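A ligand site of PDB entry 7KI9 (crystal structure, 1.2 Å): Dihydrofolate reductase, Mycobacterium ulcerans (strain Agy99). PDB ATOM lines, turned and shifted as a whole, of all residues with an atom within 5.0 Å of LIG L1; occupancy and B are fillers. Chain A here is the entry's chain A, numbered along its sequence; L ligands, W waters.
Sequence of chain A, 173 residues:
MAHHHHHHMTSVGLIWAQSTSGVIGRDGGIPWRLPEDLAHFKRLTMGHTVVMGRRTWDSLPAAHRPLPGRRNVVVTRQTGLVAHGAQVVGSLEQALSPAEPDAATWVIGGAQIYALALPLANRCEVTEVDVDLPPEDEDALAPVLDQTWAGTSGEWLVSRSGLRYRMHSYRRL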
ATOM      1  N   ILE A  15     -14.728   0.716 -22.258  1.00  0.00           N
ATOM      2  CA  ILE A  15     -15.446   1.970 -22.416  1.00  0.00           C
ATOM      3  C   ILE A  15     -16.051   2.333 -21.069  1.00  0.00           C
ATOM      4  O   ILE A  15     -16.689   1.484 -20.426  1.00  0.00           O
ATOM      5  CB  ILE A  15     -16.497   1.904 -23.551  1.00  0.00           C
ATOM      6  CG1 ILE A  15     -17.184   3.262 -23.750  1.00  0.00           C
ATOM      7  CG2 ILE A  15     -17.521   0.755 -23.365  1.00  0.00           C
ATOM      8  CD1 ILE A  15     -17.992   3.347 -25.063  1.00  0.00           C
ATOM      9  N   TRP A  16     -15.823   3.566 -20.615  1.00  0.00           N
ATOM     10  CA  TRP A  16     -16.361   4.008 -19.335  1.00  0.00           C
ATOM     11  C   TRP A  16     -16.532   5.510 -19.355  1.00  0.00           C
ATOM     12  O   TRP A  16     -15.913   6.222 -20.152  1.00  0.00           O
ATOM     13  CB  TRP A  16     -15.491   3.587 -18.137  1.00  0.00           C
ATOM     14  CG  TRP A  16     -14.185   4.321 -17.923  1.00  0.00           C
ATOM     15  CD1 TRP A  16     -13.999   5.489 -17.220  1.00  0.00           C
ATOM     16  CD2 TRP A  16     -12.861   3.883 -18.275  1.00  0.00           C
ATOM     17  NE1 TRP A  16     -12.657   5.803 -17.144  1.00  0.00           N
ATOM     18  CE2 TRP A  16     -11.942   4.837 -17.793  1.00  0.00           C
ATOM     19  CE3 TRP A  16     -12.373   2.780 -18.979  1.00  0.00           C
ATOM     20  CZ2 TRP A  16     -10.570   4.714 -17.988  1.00  0.00           C
ATOM     21  CZ3 TRP A  16     -11.024   2.662 -19.169  1.00  0.00           C
ATOM     22  CH2 TRP A  16     -10.129   3.622 -18.682  1.00  0.00           C
ATOM     23  N   ALA A  17     -17.334   6.000 -18.413  1.00  0.00           N
ATOM     24  CA  ALA A  17     -17.465   7.420 -18.120  1.00  0.00           C
ATOM     25  C   ALA A  17     -17.020   7.668 -16.686  1.00  0.00           C
ATOM     26  O   ALA A  17     -17.305   6.865 -15.788  1.00  0.00           O
ATOM     27  CB  ALA A  17     -18.920   7.872 -18.315  1.00  0.00           C
ATOM     28  N   ILE A  30     -24.474   5.098 -11.157  1.00  0.00           N
ATOM     29  CA  ILE A  30     -23.575   6.096 -11.696  1.00  0.00           C
ATOM     30  C   ILE A  30     -24.032   7.450 -11.172  1.00  0.00           C
ATOM     31  O   ILE A  30     -25.206   7.819 -11.364  1.00  0.00           O
ATOM     32  CB  ILE A  30     -23.531   6.050 -13.236  1.00  0.00           C
ATOM     33  CG1 ILE A  30     -22.923   4.704 -13.708  1.00  0.00           C
ATOM     34  CG2 ILE A  30     -22.771   7.250 -13.785  1.00  0.00           C
ATOM     35  CD1 ILE A  30     -22.982   4.466 -15.198  1.00  0.00           C
ATOM     36  N   ASP A  37     -23.450  11.243 -23.136  1.00  0.00           N
ATOM     37  CA  ASP A  37     -22.585  10.077 -22.955  1.00  0.00           C
ATOM     38  C   ASP A  37     -23.325   8.794 -23.266  1.00  0.00           C
ATOM     39  O   ASP A  37     -22.767   7.884 -23.872  1.00  0.00           O
ATOM     40  CB  ASP A  37     -21.997  10.040 -21.542  1.00  0.00           C
ATOM     41  CG  ASP A  37     -21.249   8.760 -21.308  1.00  0.00           C
ATOM     42  OD1 ASP A  37     -20.201   8.551 -21.966  1.00  0.00           O
ATOM     43  OD2 ASP A  37     -21.731   7.944 -20.492  1.00  0.00           O
ATOM     44  N   LEU A  38     -24.595   8.685 -22.875  1.00  0.00           N
ATOM     45  CA  LEU A  38     -25.367   7.501 -23.193  1.00  0.00           C
ATOM     46  C   LEU A  38     -25.450   7.299 -24.700  1.00  0.00           C
ATOM     47  O   LEU A  38     -25.301   6.182 -25.198  1.00  0.00           O
ATOM     48  CB  LEU A  38     -26.747   7.615 -22.548  1.00  0.00           C
ATOM     49  CG  LEU A  38     -27.780   6.508 -22.624  1.00  0.00           C
ATOM     50  CD1 LEU A  38     -28.702   6.660 -21.407  1.00  0.00           C
ATOM     51  CD2 LEU A  38     -28.577   6.610 -23.883  1.00  0.00           C
ATOM     52  N   HIS A  40     -23.311   8.399 -26.979  1.00  0.00           N
ATOM     53  CA  HIS A  40     -21.979   8.018 -27.420  1.00  0.00           C
ATOM     54  C   HIS A  40     -21.714   6.535 -27.158  1.00  0.00           C
ATOM     55  O   HIS A  40     -21.251   5.801 -28.044  1.00  0.00           O
ATOM     56  CB  HIS A  40     -21.003   8.905 -26.625  1.00  0.00           C
ATOM     57  CG  HIS A  40     -19.579   8.442 -26.644  1.00  0.00           C
ATOM     58  ND1 HIS A  40     -18.770   8.589 -27.736  1.00  0.00           N
ATOM     59  CD2 HIS A  40     -18.815   7.887 -25.673  1.00  0.00           C
ATOM     60  CE1 HIS A  40     -17.558   8.135 -27.441  1.00  0.00           C
ATOM     61  NE2 HIS A  40     -17.564   7.702 -26.191  1.00  0.00           N
ATOM     62  N   PHE A  41     -22.044   6.081 -25.948  1.00  0.00           N
ATOM     63  CA  PHE A  41     -21.886   4.678 -25.592  1.00  0.00           C
ATOM     64  C   PHE A  41     -22.706   3.778 -26.513  1.00  0.00           C
ATOM     65  O   PHE A  41     -22.218   2.733 -26.979  1.00  0.00           O
ATOM     66  CB  PHE A  41     -22.340   4.511 -24.128  1.00  0.00           C
ATOM     67  CG  PHE A  41     -22.446   3.081 -23.706  1.00  0.00           C
ATOM     68  CD1 PHE A  41     -21.306   2.399 -23.274  1.00  0.00           C
ATOM     69  CD2 PHE A  41     -23.654   2.398 -23.741  1.00  0.00           C
ATOM     70  CE1 PHE A  41     -21.375   1.058 -22.887  1.00  0.00           C
ATOM     71  CE2 PHE A  41     -23.741   1.056 -23.353  1.00  0.00           C
ATOM     72  CZ  PHE A  41     -22.607   0.398 -22.940  1.00  0.00           C
ATOM     73  N   LYS A  42     -23.939   4.174 -26.797  1.00  0.00           N
ATOM     74  CA  LYS A  42     -24.803   3.390 -27.679  1.00  0.00           C
ATOM     75  C   LYS A  42     -24.208   3.309 -29.088  1.00  0.00           C
ATOM     76  O   LYS A  42     -24.200   2.239 -29.703  1.00  0.00           O
ATOM     77  CB  LYS A  42     -26.204   4.018 -27.666  1.00  0.00           C
ATOM     78  CG  LYS A  42     -27.316   3.255 -28.380  1.00  0.00           C
ATOM     79  CD  LYS A  42     -28.673   3.983 -28.282  1.00  0.00           C
ATOM     80  CE  LYS A  42     -29.194   4.087 -26.851  1.00  0.00           C
ATOM     81  NZ  LYS A  42     -30.323   5.061 -26.718  1.00  0.00           N
ATOM     82  N   THR A  45     -21.160   0.908 -29.174  1.00  0.00           N
ATOM     83  CA  THR A  45     -21.355  -0.485 -28.810  1.00  0.00           C
ATOM     84  C   THR A  45     -22.440  -1.182 -29.626  1.00  0.00           C
ATOM     85  O   THR A  45     -22.487  -2.413 -29.619  1.00  0.00           O
ATOM     86  CB  THR A  45     -21.681  -0.651 -27.314  1.00  0.00           C
ATOM     87  OG1 THR A  45     -22.897   0.022 -27.000  1.00  0.00           O
ATOM     88  CG2 THR A  45     -20.542  -0.172 -26.403  1.00  0.00           C
ATOM     89  N   THR A  56     -22.678  -4.781 -12.281  1.00  0.00           N
ATOM     90  CA  THR A  56     -23.176  -3.853 -13.284  1.00  0.00           C
ATOM     91  C   THR A  56     -24.469  -4.367 -13.914  1.00  0.00           C
ATOM     92  O   THR A  56     -25.419  -3.601 -14.095  1.00  0.00           O
ATOM     93  CB  THR A  56     -22.082  -3.587 -14.328  1.00  0.00           C
ATOM     94  OG1 THR A  56     -21.010  -2.874 -13.700  1.00  0.00           O
ATOM     95  CG2 THR A  56     -22.590  -2.767 -15.492  1.00  0.00           C
ATOM     96  N   LEU A  60     -28.429  -2.314 -13.759  1.00  0.00           N
ATOM     97  CA  LEU A  60     -29.165  -1.760 -14.885  1.00  0.00           C
ATOM     98  C   LEU A  60     -30.651  -1.653 -14.535  1.00  0.00           C
ATOM     99  O   LEU A  60     -31.228  -2.617 -14.017  1.00  0.00           O
ATOM    100  CB  LEU A  60     -28.993  -2.652 -16.113  1.00  0.00           C
ATOM    101  CG  LEU A  60     -27.568  -2.845 -16.634  1.00  0.00           C
ATOM    102  CD1 LEU A  60     -27.575  -3.895 -17.743  1.00  0.00           C
ATOM    103  CD2 LEU A  60     -26.968  -1.528 -17.122  1.00  0.00           C
ATOM    104  N   PRO A  61     -31.285  -0.516 -14.786  1.00  0.00           N
ATOM    105  CA  PRO A  61     -32.747  -0.473 -14.679  1.00  0.00           C
ATOM    106  C   PRO A  61     -33.354  -1.499 -15.625  1.00  0.00           C
ATOM    107  O   PRO A  61     -32.820  -1.789 -16.695  1.00  0.00           O
ATOM    108  CB  PRO A  61     -33.097   0.957 -15.105  1.00  0.00           C
ATOM    109  CG  PRO A  61     -31.850   1.746 -14.807  1.00  0.00           C
ATOM    110  CD  PRO A  61     -30.723   0.794 -15.123  1.00  0.00           C
ATOM    111  N   HIS A  64     -33.607  -1.367 -19.385  1.00  0.00           N
ATOM    112  CA  HIS A  64     -32.377  -1.333 -20.147  1.00  0.00           C
ATOM    113  C   HIS A  64     -31.571  -2.617 -20.029  1.00  0.00           C
ATOM    114  O   HIS A  64     -30.400  -2.651 -20.431  1.00  0.00           O
ATOM    115  CB  HIS A  64     -31.511  -0.168 -19.663  1.00  0.00           C
ATOM    116  CG  HIS A  64     -32.230   1.150 -19.656  1.00  0.00           C
ATOM    117  ND1 HIS A  64     -32.695   1.736 -20.803  1.00  0.00           N
ATOM    118  CD2 HIS A  64     -32.546   1.984 -18.637  1.00  0.00           C
ATOM    119  CE1 HIS A  64     -33.275   2.892 -20.500  1.00  0.00           C
ATOM    120  NE2 HIS A  64     -33.197   3.060 -19.187  1.00  0.00           N
ATOM    121  N   LEU A  67     -29.031  -4.815 -22.613  1.00  0.00           N
ATOM    122  CA  LEU A  67     -28.807  -3.708 -23.522  1.00  0.00           C
ATOM    123  C   LEU A  67     -29.310  -4.134 -24.889  1.00  0.00           C
ATOM    124  O   LEU A  67     -28.812  -5.130 -25.432  1.00  0.00           O
ATOM    125  CB  LEU A  67     -27.315  -3.419 -23.605  1.00  0.00           C
ATOM    126  CG  LEU A  67     -26.786  -2.453 -22.569  1.00  0.00           C
ATOM    127  CD1 LEU A  67     -27.050  -2.966 -21.213  1.00  0.00           C
ATOM    128  CD2 LEU A  67     -25.282  -2.204 -22.750  1.00  0.00           C
ATOM    129  N   PRO A  68     -30.261  -3.441 -25.481  1.00  0.00           N
ATOM    130  CA  PRO A  68     -30.852  -3.952 -26.716  1.00  0.00           C
ATOM    131  C   PRO A  68     -29.886  -3.858 -27.876  1.00  0.00           C
ATOM    132  O   PRO A  68     -29.079  -2.935 -27.981  1.00  0.00           O
ATOM    133  CB  PRO A  68     -32.079  -3.057 -26.936  1.00  0.00           C
ATOM    134  CG  PRO A  68     -31.746  -1.793 -26.222  1.00  0.00           C
ATOM    135  CD  PRO A  68     -30.951  -2.218 -25.007  1.00  0.00           C
ATOM    136  N   ARG A  70     -27.385  -5.738 -28.610  1.00  0.00           N
ATOM    137  CA  ARG A  70     -26.029  -6.160 -28.305  1.00  0.00           C
ATOM    138  C   ARG A  70     -26.102  -7.512 -27.632  1.00  0.00           C
ATOM    139  O   ARG A  70     -27.070  -7.822 -26.940  1.00  0.00           O
ATOM    140  CB  ARG A  70     -25.347  -5.136 -27.389  1.00  0.00           C
ATOM    141  CG  ARG A  70     -24.871  -3.927 -28.164  1.00  0.00           C
ATOM    142  CD  ARG A  70     -24.949  -2.647 -27.375  1.00  0.00           C
ATOM    143  NE  ARG A  70     -26.321  -2.186 -27.222  1.00  0.00           N
ATOM    144  CZ  ARG A  70     -26.664  -1.097 -26.549  1.00  0.00           C
ATOM    145  NH1 ARG A  70     -25.747  -0.278 -26.050  1.00  0.00           N
ATOM    146  NH2 ARG A  70     -27.955  -0.827 -26.367  1.00  0.00           N
ATOM    147  N   ILE A 108     -17.735  -3.111 -20.559  1.00  0.00           N
ATOM    148  CA  ILE A 108     -18.528  -1.938 -20.211  1.00  0.00           C
ATOM    149  C   ILE A 108     -18.635  -1.720 -18.712  1.00  0.00           C
ATOM    150  O   ILE A 108     -19.440  -0.895 -18.279  1.00  0.00           O
ATOM    151  CB  ILE A 108     -19.912  -1.954 -20.880  1.00  0.00           C
ATOM    152  CG1 ILE A 108     -20.808  -3.043 -20.275  1.00  0.00           C
ATOM    153  CG2 ILE A 108     -19.753  -2.168 -22.403  1.00  0.00           C
ATOM    154  CD1 ILE A 108     -22.284  -2.867 -20.645  1.00  0.00           C
ATOM    155  N   GLY A 109     -17.822  -2.421 -17.923  1.00  0.00           N
ATOM    156  CA  GLY A 109     -17.729  -2.178 -16.481  1.00  0.00           C
ATOM    157  C   GLY A 109     -18.169  -3.382 -15.669  1.00  0.00           C
ATOM    158  O   GLY A 109     -18.601  -4.393 -16.222  1.00  0.00           O
ATOM    159  N   TYR A 114     -13.175  -4.107 -15.267  1.00  0.00           N
ATOM    160  CA  TYR A 114     -12.148  -3.320 -15.947  1.00  0.00           C
ATOM    161  C   TYR A 114     -10.761  -3.785 -15.544  1.00  0.00           C
ATOM    162  O   TYR A 114      -9.857  -3.863 -16.374  1.00  0.00           O
ATOM    163  CB  TYR A 114     -12.282  -1.822 -15.660  1.00  0.00           C
ATOM    164  CG  TYR A 114     -13.481  -1.128 -16.271  1.00  0.00           C
ATOM    165  CD1 TYR A 114     -13.863  -1.369 -17.591  1.00  0.00           C
ATOM    166  CD2 TYR A 114     -14.205  -0.228 -15.521  1.00  0.00           C
ATOM    167  CE1 TYR A 114     -14.968  -0.719 -18.149  1.00  0.00           C
ATOM    168  CE2 TYR A 114     -15.315   0.399 -16.052  1.00  0.00           C
ATOM    169  CZ  TYR A 114     -15.685   0.156 -17.356  1.00  0.00           C
ATOM    170  OH  TYR A 114     -16.806   0.786 -17.841  1.00  0.00           O
ATOM    171  N   THR A 127     -15.208   8.800 -21.318  1.00  0.00           N
ATOM    172  CA  THR A 127     -15.891  10.085 -21.240  1.00  0.00           C
ATOM    173  C   THR A 127     -15.533  10.685 -19.894  1.00  0.00           C
ATOM    174  O   THR A 127     -15.725  10.038 -18.857  1.00  0.00           O
ATOM    175  CB  THR A 127     -17.400   9.931 -21.346  1.00  0.00           C
ATOM    176  OG1 THR A 127     -17.692   9.259 -22.572  1.00  0.00           O
ATOM    177  CG2 THR A 127     -18.057  11.300 -21.332  1.00  0.00           C
HETATM  178  C1  LIG L   1     -24.003   5.407 -20.157  1.00  0.00           C
HETATM  179  C2  LIG L   1     -23.018   5.016 -19.027  1.00  0.00           C
HETATM  180  C3  LIG L   1     -21.722   4.504 -19.610  1.00  0.00           C
HETATM  181  C4  LIG L   1     -19.875   4.991 -20.876  1.00  0.00           C
HETATM  182  C5  LIG L   1     -20.019   2.882 -20.012  1.00  0.00           C
HETATM  183  C6  LIG L   1     -21.252   3.233 -19.423  1.00  0.00           C
HETATM  184  C7  LIG L   1     -22.903   1.586 -19.555  1.00  0.00           C
HETATM  185  C8  LIG L   1     -23.816   0.693 -18.754  1.00  0.00           C
HETATM  186  C9  LIG L   1     -24.369   1.243 -17.408  1.00  0.00           C
HETATM  187  C10 LIG L   1     -25.293   0.732 -19.278  1.00  0.00           C
HETATM  188  C11 LIG L   1     -26.605   2.447 -17.720  1.00  0.00           C
HETATM  189  C12 LIG L   1     -26.610   2.851 -16.371  1.00  0.00           C
HETATM  190  C13 LIG L   1     -27.643   3.610 -15.839  1.00  0.00           C
HETATM  191  C14 LIG L   1     -28.706   3.998 -16.641  1.00  0.00           C
HETATM  192  C15 LIG L   1     -28.713   3.607 -17.981  1.00  0.00           C
HETATM  193  C16 LIG L   1     -27.686   2.842 -18.534  1.00  0.00           C
HETATM  194  C17 LIG L   1     -28.748   1.576 -20.340  1.00  0.00           C
HETATM  195  C18 LIG L   1     -28.596   1.072 -21.789  1.00  0.00           C
HETATM  196  C19 LIG L   1     -28.246   2.208 -22.749  1.00  0.00           C
HETATM  197  C20 LIG L   1     -27.050   3.011 -22.217  1.00  0.00           C
HETATM  198  C21 LIG L   1     -27.353   3.514 -20.807  1.00  0.00           C
HETATM  199  C22 LIG L   1     -27.848   1.637 -24.071  1.00  0.00           C
HETATM  200  N1  LIG L   1     -21.016   5.370 -20.339  1.00  0.00           N
HETATM  201  N2  LIG L   1     -19.222   5.893 -21.638  1.00  0.00           N
HETATM  202  N3  LIG L   1     -19.343   3.768 -20.743  1.00  0.00           N
HETATM  203  N4  LIG L   1     -19.470   1.658 -19.854  1.00  0.00           N
HETATM  204  N5  LIG L   1     -25.533   1.712 -18.194  1.00  0.00           N
HETATM  205  N6  LIG L   1     -27.664   2.447 -19.895  1.00  0.00           N
HETATM  206  O1  LIG L   1     -21.961   2.281 -18.685  1.00  0.00           O
HETATM  207  O2  LIG L   1     -28.908   1.235 -24.837  1.00  0.00           O
HETATM  208  O3  LIG L   1     -26.726   1.523 -24.467  1.00  0.00           O
HETATM  209  P1  LG2 L   2     -18.585  -5.238 -11.434  1.00  0.00           P
HETATM  210  O1  LG2 L   2     -19.647  -4.715 -12.315  1.00  0.00           O
HETATM  211  O2  LG2 L   2     -17.172  -5.246 -11.972  1.00  0.00           O
HETATM  212  O3  LG2 L   2     -19.059  -6.723 -11.022  1.00  0.00           O
HETATM  213  C1  LG2 L   2     -18.336  -7.452 -10.009  1.00  0.00           C
HETATM  214  C2  LG2 L   2     -18.797  -8.881 -10.084  1.00  0.00           C
HETATM  215  O4  LG2 L   2     -18.235  -9.524 -11.245  1.00  0.00           O
HETATM  216  C3  LG2 L   2     -18.397  -9.763  -8.908  1.00  0.00           C
HETATM  217  O5  LG2 L   2     -19.275  -9.551  -7.805  1.00  0.00           O
HETATM  218  C4  LG2 L   2     -18.541 -11.133  -9.555  1.00  0.00           C
HETATM  219  O6  LG2 L   2     -19.904 -11.535  -9.769  1.00  0.00           O
HETATM  220  C5  LG2 L   2     -17.963 -10.876 -10.944  1.00  0.00           C
HETATM  221  N1  LG2 L   2     -16.529 -11.107 -11.017  1.00  0.00           N
HETATM  222  C6  LG2 L   2     -15.502 -10.290 -10.634  1.00  0.00           C
HETATM  223  N2  LG2 L   2     -14.307 -10.814 -10.775  1.00  0.00           N
HETATM  224  C7  LG2 L   2     -14.570 -12.062 -11.316  1.00  0.00           C
HETATM  225  C8  LG2 L   2     -13.729 -13.115 -11.728  1.00  0.00           C
HETATM  226  N3  LG2 L   2     -12.389 -13.086 -11.643  1.00  0.00           N
HETATM  227  N4  LG2 L   2     -14.319 -14.243 -12.211  1.00  0.00           N
HETATM  228  C9  LG2 L   2     -15.646 -14.287 -12.281  1.00  0.00           C
HETATM  229  N5  LG2 L   2     -16.541 -13.367 -11.925  1.00  0.00           N
HETATM  230  C10 LG2 L   2     -15.933 -12.272 -11.457  1.00  0.00           C
HETATM  231  O7  LG2 L   2     -18.645  -4.545 -10.002  1.00  0.00           O
HETATM  232  P2  LG2 L   2     -18.056  -3.184  -9.418  1.00  0.00           P
HETATM  233  O8  LG2 L   2     -16.586  -3.133  -9.623  1.00  0.00           O
HETATM  234  O9  LG2 L   2     -18.595  -3.054  -8.046  1.00  0.00           O
HETATM  235  O10 LG2 L   2     -18.665  -2.084 -10.393  1.00  0.00           O
HETATM  236  C11 LG2 L   2     -20.057  -1.720 -10.280  1.00  0.00           C
HETATM  237  C12 LG2 L   2     -20.140  -0.218 -10.190  1.00  0.00           C
HETATM  238  O11 LG2 L   2     -19.590   0.384 -11.389  1.00  0.00           O
HETATM  239  C13 LG2 L   2     -21.561   0.337 -10.081  1.00  0.00           C
HETATM  240  O12 LG2 L   2     -21.549   1.521  -9.301  1.00  0.00           O
HETATM  241  C14 LG2 L   2     -21.894   0.704 -11.522  1.00  0.00           C
HETATM  242  O13 LG2 L   2     -22.903   1.685 -11.586  1.00  0.00           O
HETATM  243  C15 LG2 L   2     -20.541   1.273 -11.933  1.00  0.00           C
HETATM  244  N6  LG2 L   2     -20.350   1.327 -13.425  1.00  0.00           N
HETATM  245  C16 LG2 L   2     -19.964   2.512 -13.939  1.00  0.00           C
HETATM  246  C17 LG2 L   2     -19.699   2.614 -15.297  1.00  0.00           C
HETATM  247  C18 LG2 L   2     -19.260   3.921 -15.892  1.00  0.00           C
HETATM  248  O14 LG2 L   2     -18.857   3.934 -17.058  1.00  0.00           O
HETATM  249  N7  LG2 L   2     -19.262   4.992 -15.121  1.00  0.00           N
HETATM  250  C19 LG2 L   2     -19.857   1.476 -16.093  1.00  0.00           C
HETATM  251  C20 LG2 L   2     -20.276   0.286 -15.530  1.00  0.00           C
HETATM  252  C21 LG2 L   2     -20.508   0.222 -14.181  1.00  0.00           C
HETATM  253  P3  LG2 L   2     -20.610 -12.519  -8.728  1.00  0.00           P
HETATM  254  O15 LG2 L   2     -19.760 -13.762  -8.652  1.00  0.00           O
HETATM  255  O16 LG2 L   2     -20.651 -11.751  -7.417  1.00  0.00           O
HETATM  256  O17 LG2 L   2     -21.964 -12.745  -9.345  1.00  0.00           O
HETATM  257  O   HOH W   1     -16.784   6.632 -23.314  1.00  0.00           O
HETATM  258  O   HOH W   2     -31.301   1.923 -24.995  1.00  0.00           O
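The side-chain hydroxyl (OG1) of Thr 45 is in hydrogen-bond range of the guanidinium group (NH1) of Arg 70 (3.0 Å).
O of Trp 16 is in hydrogen-bond range of N of Thr 127, 2.9 Å away.
OG1 of Thr 127 lies within hydrogen-bond range of OD1 of Asp 37 (2.7 Å).
OH of Tyr 114 lies close to N of Gly 109, 3.4 Å away.
The backbone carbonyl oxygen (O) of Ile 15 lies within hydrogen-bond range of the side-chain hydroxyl (OH) of Tyr 114 (2.7 Å).
The backbone carbonyl oxygen (O) of Pro 68 sits at hydrogen-bond distance from the guanidinium group (NH2) of Arg 70, 2.9 Å away.
The backbone carbonyl oxygen (O) of Phe 41 is in hydrogen-bond range of the side-chain hydroxyl (OG1) of Thr 45.
The backbone carbonyl oxygen of Ile 108 sits at hydrogen-bond distance from the side-chain hydroxyl of Tyr 114, 3.2 Å away.
Water W1 lies within hydrogen-bond range of OG1 of Thr 127 (2.9 Å), N2 of LIG L1 (3.0 Å), NE2 of His 40 (3.2 Å) and O of Trp 16 (3.3 Å).
Trp 16 touches LIG L1.
Ala 17 touches LIG L1 (N to C4, 3.7 Å).
CD1 of Ile 30 touches C2 of LIG L1, 3.9 Å away.
Leu 38 touches LIG L1.
Phe 41 touches LIG L1 (CE2 to O3, 3.2 Å).
Lys 42 touches LIG L1 (CE to O2, 3.5 Å).
CD2 of Leu 60 touches C10 of LIG L1, at 3.5 Å.
His 64 touches LIG L1 (CB to C17, 3.3 Å).
Thr 127 touches LIG L1 (OG1 to N2, 3.8 Å).
Hydrophobic or aromatic side chains that line LIG L1: Ile 15, Ala 17, Ile 30, Leu 38, Phe 41, Leu 60, His 64 and Ile 108.
Within 4 Å of LIG L1: Ile 15, Trp 16, Ala 17, Ile 30, Asp 37, Leu 38, Phe 41, Lys 42, Leu 60, His 64, Arg 70, Ile 108, Tyr 114 and Thr 127.
The nearest printed residue that does not touch LIG L1 is Pro 68 (4.02 Å).
The side-chain hydroxyl (OH) of Tyr 114 lies within hydrogen-bond range of a nitrogen (N4) of LIG L1 (3.5 Å).
The backbone carbonyl oxygen (O) of Ala 17 sits at hydrogen-bond distance from a nitrogen (N7) of LG2 L2 (2.8 Å).
The backbone carbonyl oxygen of Ile 15 lies within hydrogen-bond range of a nitrogen (N4) of LIG L1 (2.8 Å).
The backbone NH (N) of Ala 17 sits at hydrogen-bond distance from an oxygen (O14) of LG2 L2.
O3 of LIG L1 lies within salt-bridge range of NH1 of Arg 70, at 2.6 Å.
The side-chain hydroxyl of Thr 56 sits at hydrogen-bond distance from an oxygen (O1) of LG2 L2 (2.7 Å).
A nitrogen (N1) of LIG L1 lies within hydrogen-bond range of the side-chain carboxylate (OD2) of Asp 37 (2.7 Å).
O1 of LG2 L2 sits at hydrogen-bond distance from N of Thr 56 (3.0 Å).
The backbone carbonyl oxygen (O) of Ile 108 sits at hydrogen-bond distance from a nitrogen (N4) of LIG L1 (3.0 Å).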
